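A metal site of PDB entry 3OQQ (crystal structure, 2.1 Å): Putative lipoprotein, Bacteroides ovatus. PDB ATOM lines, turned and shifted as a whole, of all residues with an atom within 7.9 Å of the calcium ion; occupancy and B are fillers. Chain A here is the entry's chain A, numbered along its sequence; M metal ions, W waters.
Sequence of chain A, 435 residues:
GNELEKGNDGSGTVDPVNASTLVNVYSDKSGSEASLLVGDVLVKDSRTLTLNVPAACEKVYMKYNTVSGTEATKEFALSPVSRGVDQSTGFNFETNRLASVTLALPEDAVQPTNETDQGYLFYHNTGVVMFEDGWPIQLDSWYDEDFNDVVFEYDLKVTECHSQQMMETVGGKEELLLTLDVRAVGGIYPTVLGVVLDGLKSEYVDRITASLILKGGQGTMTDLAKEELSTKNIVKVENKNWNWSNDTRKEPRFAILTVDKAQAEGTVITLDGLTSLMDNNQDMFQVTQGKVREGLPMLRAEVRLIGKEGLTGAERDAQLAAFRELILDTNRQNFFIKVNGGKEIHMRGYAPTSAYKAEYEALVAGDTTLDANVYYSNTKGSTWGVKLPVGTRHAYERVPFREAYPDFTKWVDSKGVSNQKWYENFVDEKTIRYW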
ATOM      1  N   LEU A  22      18.191  10.492  19.431  1.00  0.00           N
ATOM      2  CA  LEU A  22      17.326   9.456  19.977  1.00  0.00           C
ATOM      3  C   LEU A  22      15.875   9.943  20.037  1.00  0.00           C
ATOM      4  O   LEU A  22      15.613  11.142  20.158  1.00  0.00           O
ATOM      5  CB  LEU A  22      17.830   8.981  21.339  1.00  0.00           C
ATOM      6  CG  LEU A  22      19.330   8.666  21.412  1.00  0.00           C
ATOM      7  CD1 LEU A  22      19.724   8.310  22.809  1.00  0.00           C
ATOM      8  CD2 LEU A  22      19.698   7.551  20.479  1.00  0.00           C
ATOM      9  N   LEU A  42      17.461   4.723  19.299  1.00  0.00           N
ATOM     10  CA  LEU A  42      18.271   5.084  18.143  1.00  0.00           C
ATOM     11  C   LEU A  42      17.607   4.500  16.895  1.00  0.00           C
ATOM     12  O   LEU A  42      17.325   3.298  16.856  1.00  0.00           O
ATOM     13  CB  LEU A  42      19.714   4.577  18.316  1.00  0.00           C
ATOM     14  CG  LEU A  42      20.634   4.580  17.090  1.00  0.00           C
ATOM     15  CD1 LEU A  42      20.925   5.991  16.608  1.00  0.00           C
ATOM     16  CD2 LEU A  42      21.914   3.857  17.397  1.00  0.00           C
ATOM     17  N   THR A 113      24.756  10.145  14.787  1.00  0.00           N
ATOM     18  CA  THR A 113      26.214  10.021  14.794  1.00  0.00           C
ATOM     19  C   THR A 113      26.583   9.668  16.210  1.00  0.00           C
ATOM     20  O   THR A 113      25.729   9.786  17.098  1.00  0.00           O
ATOM     21  CB  THR A 113      26.991  11.248  14.290  1.00  0.00           C
ATOM     22  OG1 THR A 113      26.721  12.377  15.123  1.00  0.00           O
ATOM     23  CG2 THR A 113      26.758  11.552  12.809  1.00  0.00           C
ATOM     24  N   ASN A 114      27.832   9.250  16.457  1.00  0.00           N
ATOM     25  CA  ASN A 114      28.242   8.916  17.818  1.00  0.00           C
ATOM     26  C   ASN A 114      28.269  10.190  18.731  1.00  0.00           C
ATOM     27  O   ASN A 114      28.303  10.072  19.949  1.00  0.00           O
ATOM     28  CB  ASN A 114      29.560   8.168  17.829  1.00  0.00           C
ATOM     29  CG  ASN A 114      29.402   6.696  17.479  1.00  0.00           C
ATOM     30  OD1 ASN A 114      28.647   5.962  18.118  1.00  0.00           O
ATOM     31  ND2 ASN A 114      30.118   6.210  16.458  1.00  0.00           N
ATOM     32  N   GLU A 115      28.193  11.392  18.108  1.00  0.00           N
ATOM     33  CA  GLU A 115      28.132  12.687  18.769  1.00  0.00           C
ATOM     34  C   GLU A 115      26.711  12.974  19.305  1.00  0.00           C
ATOM     35  O   GLU A 115      26.576  13.687  20.311  1.00  0.00           O
ATOM     36  CB  GLU A 115      28.576  13.808  17.767  1.00  0.00           C
ATOM     37  CG  GLU A 115      28.474  15.248  18.258  1.00  0.00           C
ATOM     38  CD  GLU A 115      28.952  16.343  17.321  1.00  0.00           C
ATOM     39  OE1 GLU A 115      28.598  16.328  16.115  1.00  0.00           O
ATOM     40  OE2 GLU A 115      29.633  17.273  17.812  1.00  0.00           O
ATOM     41  N   THR A 116      25.643  12.391  18.660  1.00  0.00           N
ATOM     42  CA  THR A 116      24.235  12.631  18.980  1.00  0.00           C
ATOM     43  C   THR A 116      23.407  11.398  19.465  1.00  0.00           C
ATOM     44  O   THR A 116      22.221  11.573  19.781  1.00  0.00           O
ATOM     45  CB  THR A 116      23.536  13.215  17.738  1.00  0.00           C
ATOM     46  OG1 THR A 116      23.508  12.229  16.707  1.00  0.00           O
ATOM     47  CG2 THR A 116      24.228  14.465  17.216  1.00  0.00           C
ATOM     48  N   ASP A 117      24.007  10.192  19.552  1.00  0.00           N
ATOM     49  CA  ASP A 117      23.259   8.978  19.949  1.00  0.00           C
ATOM     50  C   ASP A 117      23.599   8.465  21.374  1.00  0.00           C
ATOM     51  O   ASP A 117      23.338   7.296  21.673  1.00  0.00           O
ATOM     52  CB  ASP A 117      23.551   7.856  18.919  1.00  0.00           C
ATOM     53  CG  ASP A 117      24.970   7.272  18.958  1.00  0.00           C
ATOM     54  OD1 ASP A 117      25.815   7.790  19.730  1.00  0.00           O
ATOM     55  OD2 ASP A 117      25.234   6.299  18.220  1.00  0.00           O
ATOM     56  N   GLN A 118      24.244   9.282  22.203  1.00  0.00           N
ATOM     57  CA  GLN A 118      24.694   8.828  23.522  1.00  0.00           C
ATOM     58  C   GLN A 118      23.537   8.742  24.532  1.00  0.00           C
ATOM     59  O   GLN A 118      23.289   9.692  25.280  1.00  0.00           O
ATOM     60  CB  GLN A 118      25.836   9.714  24.051  1.00  0.00           C
ATOM     61  CG  GLN A 118      27.114   9.650  23.215  1.00  0.00           C
ATOM     62  CD  GLN A 118      28.059  10.772  23.561  1.00  0.00           C
ATOM     63  OE1 GLN A 118      28.310  11.078  24.734  1.00  0.00           O
ATOM     64  NE2 GLN A 118      28.614  11.417  22.546  1.00  0.00           N
ATOM     65  N   GLY A 119      22.855   7.599  24.540  1.00  0.00           N
ATOM     66  CA  GLY A 119      21.726   7.358  25.420  1.00  0.00           C
ATOM     67  C   GLY A 119      21.294   5.911  25.400  1.00  0.00           C
ATOM     68  O   GLY A 119      21.447   5.221  24.388  1.00  0.00           O
ATOM     69  N   SER A 163      26.687   0.001  25.631  1.00  0.00           N
ATOM     70  CA  SER A 163      27.532   1.063  25.058  1.00  0.00           C
ATOM     71  C   SER A 163      26.980   1.600  23.706  1.00  0.00           C
ATOM     72  O   SER A 163      27.253   2.751  23.346  1.00  0.00           O
ATOM     73  CB  SER A 163      28.956   0.555  24.874  1.00  0.00           C
ATOM     74  OG  SER A 163      29.842   1.627  24.612  1.00  0.00           O
ATOM     75  N   GLN A 164      26.225   0.761  22.977  1.00  0.00           N
ATOM     76  CA  GLN A 164      25.641   1.073  21.673  1.00  0.00           C
ATOM     77  C   GLN A 164      24.361   0.258  21.442  1.00  0.00           C
ATOM     78  O   GLN A 164      24.303  -0.922  21.799  1.00  0.00           O
ATOM     79  CB  GLN A 164      26.695   0.770  20.572  1.00  0.00           C
ATOM     80  CG  GLN A 164      26.292   1.159  19.146  1.00  0.00           C
ATOM     81  CD  GLN A 164      26.053   2.638  18.882  1.00  0.00           C
ATOM     82  OE1 GLN A 164      26.764   3.534  19.366  1.00  0.00           O
ATOM     83  NE2 GLN A 164      25.100   2.931  18.018  1.00  0.00           N
ATOM     84  N   GLN A 165      23.368   0.889  20.815  1.00  0.00           N
ATOM     85  CA  GLN A 165      22.097   0.236  20.489  1.00  0.00           C
ATOM     86  C   GLN A 165      22.217  -0.586  19.204  1.00  0.00           C
ATOM     87  O   GLN A 165      23.155  -0.383  18.429  1.00  0.00           O
ATOM     88  CB  GLN A 165      20.975   1.283  20.363  1.00  0.00           C
ATOM     89  CG  GLN A 165      20.666   2.008  21.676  1.00  0.00           C
ATOM     90  CD  GLN A 165      19.446   2.891  21.605  1.00  0.00           C
ATOM     91  OE1 GLN A 165      18.474   2.592  20.914  1.00  0.00           O
ATOM     92  NE2 GLN A 165      19.449   3.958  22.386  1.00  0.00           N
HETATM   93 CA    CA M   1      27.294   5.822  19.798  1.00  0.00          CA
HETATM   94  O   HOH W   1      28.328   7.318  20.995  1.00  0.00           O
HETATM   95  O   HOH W   2      25.884   4.915  21.853  1.00  0.00           O
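O of Asn 114 is in hydrogen-bond range of NE2 of Gln 118, at 2.9 Å.
Of the 12 residues printed, 3 come within 4 Å of the calcium ion. The nearest printed residue that does not touch the calcium ion is Ser 163 (4.7 Å).
OD1 of Asn 114 is bound to the calcium ion. Water W1 binds the calcium ion (2.2 Å). The calcium ion is bound by OE1 of Gln 164 (2.4 Å). The calcium ion is bound by OD1 of Asp 117 (2.5 Å). The calcium ion is bound by OD2 of Asp 117, 2.6 Å away. The calcium ion is bound by water W2, 2.7 Å away.
Water W2 lies within hydrogen-bond range of O of Ser 163 (3.0 Å) and O of Asp 117 (3.5 Å).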
